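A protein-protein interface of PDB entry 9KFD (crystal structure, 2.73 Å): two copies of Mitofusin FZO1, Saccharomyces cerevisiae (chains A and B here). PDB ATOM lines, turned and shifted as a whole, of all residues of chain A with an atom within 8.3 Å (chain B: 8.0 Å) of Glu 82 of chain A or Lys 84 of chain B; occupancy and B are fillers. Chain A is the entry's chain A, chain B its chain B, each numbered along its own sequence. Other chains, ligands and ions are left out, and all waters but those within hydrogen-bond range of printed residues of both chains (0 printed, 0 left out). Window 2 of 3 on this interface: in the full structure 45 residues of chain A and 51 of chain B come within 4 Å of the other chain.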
ATOM      1  N   PRO A  46     -23.431  -4.536  14.864  1.00  0.00           N
ATOM      2  CA  PRO A  46     -23.299  -3.102  15.150  1.00  0.00           C
ATOM      3  C   PRO A  46     -23.364  -2.249  13.891  1.00  0.00           C
ATOM      4  O   PRO A  46     -22.954  -2.664  12.804  1.00  0.00           O
ATOM      5  CB  PRO A  46     -21.925  -3.005  15.819  1.00  0.00           C
ATOM      6  CG  PRO A  46     -21.718  -4.354  16.428  1.00  0.00           C
ATOM      7  CD  PRO A  46     -22.337  -5.321  15.461  1.00  0.00           C
ATOM      8  N   ILE A  47     -23.895  -1.036  14.056  1.00  0.00           N
ATOM      9  CA  ILE A  47     -24.071  -0.095  12.955  1.00  0.00           C
ATOM     10  C   ILE A  47     -22.911   0.893  12.967  1.00  0.00           C
ATOM     11  O   ILE A  47     -22.033   0.821  13.834  1.00  0.00           O
ATOM     12  CB  ILE A  47     -25.462   0.582  13.031  1.00  0.00           C
ATOM     13  CG1 ILE A  47     -25.591   1.614  14.164  1.00  0.00           C
ATOM     14  CG2 ILE A  47     -26.555  -0.469  13.178  1.00  0.00           C
ATOM     15  CD1 ILE A  47     -25.154   3.022  13.828  1.00  0.00           C
ATOM     16  N   ILE A  49     -21.456   4.605  13.348  1.00  0.00           N
ATOM     17  CA  ILE A  49     -21.736   5.899  13.946  1.00  0.00           C
ATOM     18  C   ILE A  49     -20.695   6.950  13.574  1.00  0.00           C
ATOM     19  O   ILE A  49     -21.041   8.130  13.450  1.00  0.00           O
ATOM     20  CB  ILE A  49     -21.852   5.755  15.478  1.00  0.00           C
ATOM     21  CG1 ILE A  49     -23.120   4.984  15.832  1.00  0.00           C
ATOM     22  CG2 ILE A  49     -21.852   7.109  16.173  1.00  0.00           C
ATOM     23  CD1 ILE A  49     -22.888   3.858  16.795  1.00  0.00           C
ATOM     24  N   ALA A  50     -19.445   6.551  13.356  1.00  0.00           N
ATOM     25  CA  ALA A  50     -18.385   7.504  13.067  1.00  0.00           C
ATOM     26  C   ALA A  50     -18.630   8.219  11.741  1.00  0.00           C
ATOM     27  O   ALA A  50     -19.262   7.686  10.825  1.00  0.00           O
ATOM     28  CB  ALA A  50     -17.031   6.799  13.034  1.00  0.00           C
ATOM     29  N   GLY A  78     -13.127  12.927  19.063  1.00  0.00           N
ATOM     30  CA  GLY A  78     -13.081  11.720  18.259  1.00  0.00           C
ATOM     31  C   GLY A  78     -12.669  10.483  19.031  1.00  0.00           C
ATOM     32  O   GLY A  78     -13.441   9.525  19.125  1.00  0.00           O
ATOM     33  N   PHE A  79     -11.436  10.486  19.552  1.00  0.00           N
ATOM     34  CA  PHE A  79     -10.901   9.440  20.423  1.00  0.00           C
ATOM     35  C   PHE A  79     -10.657   8.131  19.675  1.00  0.00           C
ATOM     36  O   PHE A  79     -10.037   7.210  20.218  1.00  0.00           O
ATOM     37  CB  PHE A  79     -11.833   9.218  21.618  1.00  0.00           C
ATOM     38  CG  PHE A  79     -11.926  10.402  22.538  1.00  0.00           C
ATOM     39  CD1 PHE A  79     -10.925  11.360  22.565  1.00  0.00           C
ATOM     40  CD2 PHE A  79     -13.003  10.544  23.395  1.00  0.00           C
ATOM     41  CE1 PHE A  79     -11.009  12.447  23.418  1.00  0.00           C
ATOM     42  CE2 PHE A  79     -13.094  11.628  24.246  1.00  0.00           C
ATOM     43  CZ  PHE A  79     -12.095  12.579  24.259  1.00  0.00           C
ATOM     44  N   ASN A  80     -11.140   8.044  18.434  1.00  0.00           N
ATOM     45  CA  ASN A  80     -10.830   6.938  17.524  1.00  0.00           C
ATOM     46  C   ASN A  80     -11.269   5.588  18.089  1.00  0.00           C
ATOM     47  O   ASN A  80     -10.582   4.577  17.928  1.00  0.00           O
ATOM     48  CB  ASN A  80      -9.339   6.916  17.174  1.00  0.00           C
ATOM     49  CG  ASN A  80      -8.940   8.059  16.262  1.00  0.00           C
ATOM     50  OD1 ASN A  80      -9.679   9.032  16.108  1.00  0.00           O
ATOM     51  ND2 ASN A  80      -7.768   7.945  15.648  1.00  0.00           N
ATOM     52  N   ILE A  81     -12.427   5.563  18.750  1.00  0.00           N
ATOM     53  CA  ILE A  81     -12.978   4.299  19.223  1.00  0.00           C
ATOM     54  C   ILE A  81     -13.417   3.465  18.029  1.00  0.00           C
ATOM     55  O   ILE A  81     -13.926   3.994  17.031  1.00  0.00           O
ATOM     56  CB  ILE A  81     -14.150   4.521  20.196  1.00  0.00           C
ATOM     57  CG1 ILE A  81     -13.905   5.712  21.128  1.00  0.00           C
ATOM     58  CG2 ILE A  81     -14.414   3.265  21.007  1.00  0.00           C
ATOM     59  CD1 ILE A  81     -14.496   7.013  20.634  1.00  0.00           C
ATOM     60  N   GLU A  82     -13.222   2.153  18.123  1.00  0.00           N
ATOM     61  CA  GLU A  82     -13.602   1.268  17.036  1.00  0.00           C
ATOM     62  C   GLU A  82     -15.123   1.152  16.952  1.00  0.00           C
ATOM     63  O   GLU A  82     -15.866   1.658  17.798  1.00  0.00           O
ATOM     64  CB  GLU A  82     -12.955  -0.105  17.212  1.00  0.00           C
ATOM     65  CG  GLU A  82     -11.492  -0.140  16.793  1.00  0.00           C
ATOM     66  CD  GLU A  82     -10.780  -1.396  17.251  1.00  0.00           C
ATOM     67  OE1 GLU A  82      -9.545  -1.342  17.451  1.00  0.00           O
ATOM     68  OE2 GLU A  82     -11.451  -2.438  17.404  1.00  0.00           O
ATOM     69  N   LYS A  83     -15.583   0.466  15.903  1.00  0.00           N
ATOM     70  CA  LYS A  83     -17.008   0.449  15.583  1.00  0.00           C
ATOM     71  C   LYS A  83     -17.822  -0.242  16.670  1.00  0.00           C
ATOM     72  O   LYS A  83     -18.839   0.293  17.130  1.00  0.00           O
ATOM     73  CB  LYS A  83     -17.226  -0.237  14.236  1.00  0.00           C
ATOM     74  CG  LYS A  83     -18.568  -0.940  14.117  1.00  0.00           C
ATOM     75  CD  LYS A  83     -18.610  -1.839  12.904  1.00  0.00           C
ATOM     76  CE  LYS A  83     -19.807  -2.770  12.960  1.00  0.00           C
ATOM     77  NZ  LYS A  83     -20.076  -3.441  11.658  1.00  0.00           N
ATOM     78  N   LYS A  84     -17.392  -1.433  17.095  1.00  0.00           N
ATOM     79  CA  LYS A  84     -18.216  -2.241  17.990  1.00  0.00           C
ATOM     80  C   LYS A  84     -18.411  -1.563  19.341  1.00  0.00           C
ATOM     81  O   LYS A  84     -19.493  -1.649  19.934  1.00  0.00           O
ATOM     82  CB  LYS A  84     -17.596  -3.626  18.168  1.00  0.00           C
ATOM     83  CG  LYS A  84     -18.597  -4.700  18.564  1.00  0.00           C
ATOM     84  CD  LYS A  84     -18.014  -6.094  18.402  1.00  0.00           C
ATOM     85  CE  LYS A  84     -18.765  -6.881  17.336  1.00  0.00           C
ATOM     86  NZ  LYS A  84     -19.804  -7.775  17.921  1.00  0.00           N
ATOM     87  N   ALA A  85     -17.380  -0.881  19.843  1.00  0.00           N
ATOM     88  CA  ALA A  85     -17.504  -0.218  21.138  1.00  0.00           C
ATOM     89  C   ALA A  85     -18.436   0.986  21.058  1.00  0.00           C
ATOM     90  O   ALA A  85     -19.185   1.260  22.003  1.00  0.00           O
ATOM     91  CB  ALA A  85     -16.128   0.200  21.651  1.00  0.00           C
ATOM     92  N   LEU A  86     -18.406   1.713  19.938  1.00  0.00           N
ATOM     93  CA  LEU A  86     -19.290   2.866  19.783  1.00  0.00           C
ATOM     94  C   LEU A  86     -20.753   2.442  19.742  1.00  0.00           C
ATOM     95  O   LEU A  86     -21.622   3.128  20.293  1.00  0.00           O
ATOM     96  CB  LEU A  86     -18.928   3.644  18.518  1.00  0.00           C
ATOM     97  CG  LEU A  86     -17.753   4.618  18.605  1.00  0.00           C
ATOM     98  CD1 LEU A  86     -17.530   5.304  17.266  1.00  0.00           C
ATOM     99  CD2 LEU A  86     -17.996   5.644  19.699  1.00  0.00           C
ATOM    100  N   SER A  87     -21.047   1.313  19.090  1.00  0.00           N
ATOM    101  CA  SER A  87     -22.431   0.868  18.978  1.00  0.00           C
ATOM    102  C   SER A  87     -22.996   0.434  20.324  1.00  0.00           C
ATOM    103  O   SER A  87     -24.200   0.585  20.564  1.00  0.00           O
ATOM    104  CB  SER A  87     -22.541  -0.272  17.968  1.00  0.00           C
ATOM    105  OG  SER A  87     -22.476  -1.530  18.616  1.00  0.00           O
ATOM    106  N   LYS A  88     -22.154  -0.110  21.207  1.00  0.00           N
ATOM    107  CA  LYS A  88     -22.621  -0.443  22.548  1.00  0.00           C
ATOM    108  C   LYS A  88     -22.972   0.810  23.339  1.00  0.00           C
ATOM    109  O   LYS A  88     -23.915   0.793  24.139  1.00  0.00           O
ATOM    110  CB  LYS A  88     -21.565  -1.266  23.285  1.00  0.00           C
ATOM    111  CG  LYS A  88     -21.699  -2.768  23.082  1.00  0.00           C
ATOM    112  CD  LYS A  88     -21.449  -3.537  24.372  1.00  0.00           C
ATOM    113  CE  LYS A  88     -22.654  -3.474  25.300  1.00  0.00           C
ATOM    114  NZ  LYS A  88     -22.421  -4.230  26.563  1.00  0.00           N
ATOM    115  N   LEU A  89     -22.230   1.902  23.131  1.00  0.00           N
ATOM    116  CA  LEU A  89     -22.594   3.175  23.744  1.00  0.00           C
ATOM    117  C   LEU A  89     -23.808   3.792  23.065  1.00  0.00           C
ATOM    118  O   LEU A  89     -24.587   4.502  23.711  1.00  0.00           O
ATOM    119  CB  LEU A  89     -21.415   4.144  23.687  1.00  0.00           C
ATOM    120  CG  LEU A  89     -20.175   3.787  24.508  1.00  0.00           C
ATOM    121  CD1 LEU A  89     -19.133   4.882  24.381  1.00  0.00           C
ATOM    122  CD2 LEU A  89     -20.544   3.559  25.963  1.00  0.00           C
ATOM    123  N   ASN B  42       0.573   2.132  27.396  1.00  0.00           N
ATOM    124  CA  ASN B  42      -0.857   2.094  27.104  1.00  0.00           C
ATOM    125  C   ASN B  42      -1.127   2.002  25.608  1.00  0.00           C
ATOM    126  O   ASN B  42      -2.158   1.459  25.195  1.00  0.00           O
ATOM    127  CB  ASN B  42      -1.537   3.331  27.693  1.00  0.00           C
ATOM    128  CG  ASN B  42      -3.046   3.288  27.557  1.00  0.00           C
ATOM    129  OD1 ASN B  42      -3.703   2.382  28.070  1.00  0.00           O
ATOM    130  ND2 ASN B  42      -3.605   4.271  26.859  1.00  0.00           N
ATOM    131  N   ARG B  45      -0.122  -1.887  24.524  1.00  0.00           N
ATOM    132  CA  ARG B  45      -1.116  -2.755  25.143  1.00  0.00           C
ATOM    133  C   ARG B  45      -1.922  -1.962  26.163  1.00  0.00           C
ATOM    134  O   ARG B  45      -1.346  -1.339  27.064  1.00  0.00           O
ATOM    135  CB  ARG B  45      -0.462  -3.969  25.806  1.00  0.00           C
ATOM    136  CG  ARG B  45       0.855  -3.673  26.483  1.00  0.00           C
ATOM    137  CD  ARG B  45       1.679  -4.933  26.677  1.00  0.00           C
ATOM    138  NE  ARG B  45       3.102  -4.636  26.777  1.00  0.00           N
ATOM    139  CZ  ARG B  45       3.866  -4.273  25.757  1.00  0.00           C
ATOM    140  NH1 ARG B  45       3.384  -4.191  24.528  1.00  0.00           N
ATOM    141  NH2 ARG B  45       5.146  -3.987  25.973  1.00  0.00           N
ATOM    142  N   PRO B  46      -3.250  -1.959  26.047  1.00  0.00           N
ATOM    143  CA  PRO B  46      -4.082  -1.195  26.984  1.00  0.00           C
ATOM    144  C   PRO B  46      -3.903  -1.656  28.424  1.00  0.00           C
ATOM    145  O   PRO B  46      -3.392  -2.742  28.700  1.00  0.00           O
ATOM    146  CB  PRO B  46      -5.507  -1.468  26.488  1.00  0.00           C
ATOM    147  CG  PRO B  46      -5.341  -1.812  25.040  1.00  0.00           C
ATOM    148  CD  PRO B  46      -4.043  -2.554  24.957  1.00  0.00           C
ATOM    149  N   ILE B  47      -4.355  -0.815  29.349  1.00  0.00           N
ATOM    150  CA  ILE B  47      -4.180  -1.052  30.773  1.00  0.00           C
ATOM    151  C   ILE B  47      -5.548  -1.260  31.418  1.00  0.00           C
ATOM    152  O   ILE B  47      -6.588  -0.934  30.850  1.00  0.00           O
ATOM    153  CB  ILE B  47      -3.410   0.096  31.459  1.00  0.00           C
ATOM    154  CG1 ILE B  47      -4.119   1.433  31.232  1.00  0.00           C
ATOM    155  CG2 ILE B  47      -1.996   0.174  30.928  1.00  0.00           C
ATOM    156  CD1 ILE B  47      -3.356   2.620  31.786  1.00  0.00           C
ATOM    157  N   ILE B  81     -18.549  -0.308  28.268  1.00  0.00           N
ATOM    158  CA  ILE B  81     -17.276  -0.028  27.618  1.00  0.00           C
ATOM    159  C   ILE B  81     -16.291  -1.121  27.996  1.00  0.00           C
ATOM    160  O   ILE B  81     -16.245  -1.557  29.151  1.00  0.00           O
ATOM    161  CB  ILE B  81     -16.712   1.356  28.004  1.00  0.00           C
ATOM    162  CG1 ILE B  81     -17.830   2.395  28.120  1.00  0.00           C
ATOM    163  CG2 ILE B  81     -15.680   1.807  26.991  1.00  0.00           C
ATOM    164  CD1 ILE B  81     -18.331   2.611  29.534  1.00  0.00           C
ATOM    165  N   GLU B  82     -15.498  -1.553  27.029  1.00  0.00           N
ATOM    166  CA  GLU B  82     -14.526  -2.600  27.273  1.00  0.00           C
ATOM    167  C   GLU B  82     -13.123  -2.011  27.342  1.00  0.00           C
ATOM    168  O   GLU B  82     -12.912  -0.808  27.165  1.00  0.00           O
ATOM    169  CB  GLU B  82     -14.625  -3.688  26.204  1.00  0.00           C
ATOM    170  CG  GLU B  82     -15.917  -4.532  26.199  1.00  0.00           C
ATOM    171  CD  GLU B  82     -16.316  -5.169  27.541  1.00  0.00           C
ATOM    172  OE1 GLU B  82     -16.072  -4.602  28.626  1.00  0.00           O
ATOM    173  OE2 GLU B  82     -16.900  -6.272  27.501  1.00  0.00           O
ATOM    174  N   LYS B  83     -12.165  -2.901  27.601  1.00  0.00           N
ATOM    175  CA  LYS B  83     -10.791  -2.503  27.895  1.00  0.00           C
ATOM    176  C   LYS B  83     -10.191  -1.601  26.824  1.00  0.00           C
ATOM    177  O   LYS B  83      -9.640  -0.538  27.133  1.00  0.00           O
ATOM    178  CB  LYS B  83      -9.932  -3.748  28.068  1.00  0.00           C
ATOM    179  CG  LYS B  83      -8.546  -3.427  28.524  1.00  0.00           C
ATOM    180  CD  LYS B  83      -7.880  -4.577  29.196  1.00  0.00           C
ATOM    181  CE  LYS B  83      -6.456  -4.626  28.680  1.00  0.00           C
ATOM    182  NZ  LYS B  83      -5.444  -4.035  29.538  1.00  0.00           N
ATOM    183  N   LYS B  84     -10.231  -2.042  25.565  1.00  0.00           N
ATOM    184  CA  LYS B  84      -9.616  -1.280  24.482  1.00  0.00           C
ATOM    185  C   LYS B  84     -10.139   0.152  24.457  1.00  0.00           C
ATOM    186  O   LYS B  84      -9.359   1.112  24.453  1.00  0.00           O
ATOM    187  CB  LYS B  84      -9.870  -1.993  23.147  1.00  0.00           C
ATOM    188  CG  LYS B  84      -9.087  -1.483  21.923  1.00  0.00           C
ATOM    189  CD  LYS B  84      -9.626  -0.172  21.351  1.00  0.00           C
ATOM    190  CE  LYS B  84     -11.150  -0.170  21.256  1.00  0.00           C
ATOM    191  NZ  LYS B  84     -11.650   0.819  20.263  1.00  0.00           N
ATOM    192  N   ALA B  85     -11.466   0.311  24.451  1.00  0.00           N
ATOM    193  CA  ALA B  85     -12.059   1.639  24.307  1.00  0.00           C
ATOM    194  C   ALA B  85     -11.739   2.530  25.503  1.00  0.00           C
ATOM    195  O   ALA B  85     -11.464   3.724  25.338  1.00  0.00           O
ATOM    196  CB  ALA B  85     -13.569   1.521  24.115  1.00  0.00           C
ATOM    197  N   LEU B  86     -11.776   1.968  26.715  1.00  0.00           N
ATOM    198  CA  LEU B  86     -11.446   2.754  27.901  1.00  0.00           C
ATOM    199  C   LEU B  86     -10.014   3.271  27.843  1.00  0.00           C
ATOM    200  O   LEU B  86      -9.741   4.409  28.243  1.00  0.00           O
ATOM    201  CB  LEU B  86     -11.659   1.920  29.165  1.00  0.00           C
ATOM    202  CG  LEU B  86     -13.104   1.674  29.597  1.00  0.00           C
ATOM    203  CD1 LEU B  86     -13.206   0.415  30.446  1.00  0.00           C
ATOM    204  CD2 LEU B  86     -13.643   2.879  30.349  1.00  0.00           C
ATOM    205  N   SER B  87      -9.085   2.450  27.346  1.00  0.00           N
ATOM    206  CA  SER B  87      -7.694   2.883  27.261  1.00  0.00           C
ATOM    207  C   SER B  87      -7.517   4.025  26.269  1.00  0.00           C
ATOM    208  O   SER B  87      -6.672   4.901  26.481  1.00  0.00           O
ATOM    209  CB  SER B  87      -6.799   1.705  26.884  1.00  0.00           C
ATOM    210  OG  SER B  87      -6.569   1.658  25.486  1.00  0.00           O
ATOM    211  N   LYS B  88      -8.292   4.030  25.182  1.00  0.00           N
ATOM    212  CA  LYS B  88      -8.252   5.163  24.264  1.00  0.00           C
ATOM    213  C   LYS B  88      -8.791   6.423  24.930  1.00  0.00           C
ATOM    214  O   LYS B  88      -8.295   7.527  24.679  1.00  0.00           O
ATOM    215  CB  LYS B  88      -9.038   4.840  22.994  1.00  0.00           C
ATOM    216  CG  LYS B  88      -8.350   3.828  22.089  1.00  0.00           C
ATOM    217  CD  LYS B  88      -8.684   4.064  20.626  1.00  0.00           C
ATOM    218  CE  LYS B  88      -8.540   2.784  19.822  1.00  0.00           C
ATOM    219  NZ  LYS B  88      -9.229   2.845  18.503  1.00  0.00           N
ATOM    220  N   LEU B  89      -9.805   6.273  25.783  1.00  0.00           N
ATOM    221  CA  LEU B  89     -10.309   7.410  26.545  1.00  0.00           C
ATOM    222  C   LEU B  89      -9.273   7.890  27.553  1.00  0.00           C
ATOM    223  O   LEU B  89      -9.080   9.098  27.731  1.00  0.00           O
ATOM    224  CB  LEU B  89     -11.605   7.019  27.251  1.00  0.00           C
ATOM    225  CG  LEU B  89     -12.786   6.726  26.323  1.00  0.00           C
ATOM    226  CD1 LEU B  89     -13.980   6.200  27.098  1.00  0.00           C
ATOM    227  CD2 LEU B  89     -13.163   7.968  25.550  1.00  0.00           C
ATOM    228  N   PHE B  90      -8.590   6.953  28.210  1.00  0.00           N
ATOM    229  CA  PHE B  90      -7.595   7.298  29.216  1.00  0.00           C
ATOM    230  C   PHE B  90      -6.332   7.888  28.607  1.00  0.00           C
ATOM    231  O   PHE B  90      -5.601   8.604  29.300  1.00  0.00           O
ATOM    232  CB  PHE B  90      -7.260   6.055  30.038  1.00  0.00           C
ATOM    233  CG  PHE B  90      -6.226   6.280  31.105  1.00  0.00           C
ATOM    234  CD1 PHE B  90      -6.571   6.871  32.309  1.00  0.00           C
ATOM    235  CD2 PHE B  90      -4.917   5.865  30.920  1.00  0.00           C
ATOM    236  CE1 PHE B  90      -5.625   7.069  33.298  1.00  0.00           C
ATOM    237  CE2 PHE B  90      -3.966   6.058  31.906  1.00  0.00           C
ATOM    238  CZ  PHE B  90      -4.322   6.661  33.095  1.00  0.00           C
ATOM    239  N   HIS B  91      -6.057   7.606  27.331  1.00  0.00           N
ATOM    240  CA  HIS B  91      -4.877   8.178  26.691  1.00  0.00           C
ATOM    241  C   HIS B  91      -4.962   9.697  26.637  1.00  0.00           C
ATOM    242  O   HIS B  91      -3.967  10.391  26.876  1.00  0.00           O
ATOM    243  CB  HIS B  91      -4.705   7.605  25.286  1.00  0.00           C
ATOM    244  CG  HIS B  91      -3.651   8.298  24.483  1.00  0.00           C
ATOM    245  ND1 HIS B  91      -3.936   9.337  23.621  1.00  0.00           N
ATOM    246  CD2 HIS B  91      -2.313   8.111  24.416  1.00  0.00           C
ATOM    247  CE1 HIS B  91      -2.818   9.754  23.054  1.00  0.00           C
ATOM    248  NE2 HIS B  91      -1.818   9.027  23.520  1.00  0.00           N
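The backbone carbonyl oxygen of Asn 80 of chain A sits close to the side-chain amino group of Lys 88 of chain B, 2.3 Å away. NZ of Lys 84 of chain B sits close to N of Glu 82 of chain A, at 3.0 Å.
OG of Ser 87 of chain B lies within hydrogen-bond range of O of Lys 84 of chain B (3.0 Å).
Lys 88 of chain B touches Phe 79 of chain A. Phe 79 of chain A touches Leu 89 of chain B. Ile 81 of chain A touches Lys 84 of chain B. CG2 of Ile 81 of chain A touches CB of Ala 85 of chain B, 3.7 Å away. Ala 85 of chain A touches Ala 85 of chain B (CB to CB, 3.8 Å). Ile 81 of chain B touches Leu 89 of chain A.
Glu 82 of chain A touches just one residue of chain B: Lys 84. Of chain A, only Ile 81 and Glu 82 come within 4 Å of Lys 84 of chain B. Of the printed residues of chain A, Ala 85 of chain B touches Ile 81 and Ala 85. Of the printed residues of chain B, Phe 79 of chain A touches Lys 88 (3.4 Å) and Leu 89 (3.4 Å). Of the printed residues of chain A, Ile 81 of chain B touches Leu 89. Asn 42 of chain B touches none of the printed residues of chain A. The nearest printed residue of chain B that does not touch Ala 85 of chain A is Lys 84 of chain B (4.7 Å).
Of the 15 printed residues of chain B, 5 touch a printed residue of chain A. Of the 16 printed residues of chain A, 6 touch a printed residue of chain B. Hydrophobic or aromatic side chains of chain A that line the printed part of chain B: Phe 79, Ile 81, Ala 85 and Leu 89. Among the printed residues, 8 pairs touch across the chains. Among the printed residues, no Asp or Glu carboxylate lies within 4 Å of a Lys or Arg side-chain nitrogen of the other chain.
Ile 81 of chain A touches Lys 84 of chain B, but with the chains exchanged Lys 84 of chain A does not touch Ile 81 of chain B (8.2 Å). Ile 81 of chain A touches Ala 85 of chain B, but with the chains exchanged Ala 85 of chain A does not touch Ile 81 of chain B (5.6 Å). Ala 85 of chain B touches its own counterpart, Ala 85 of chain A. Leu 89 of chain A touches Ile 81 of chain B, but with the chains exchanged Ile 81 of chain A does not touch Leu 89 of chain B (5.0 Å). Positions printed for both chains: 46, 47, 81, 82, 83, 84, 85, 86, 87, 88 and 89. Of the 8 pairs that touch across the chains among the printed residues, 1 has its exchanged pair printed and touching as well.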
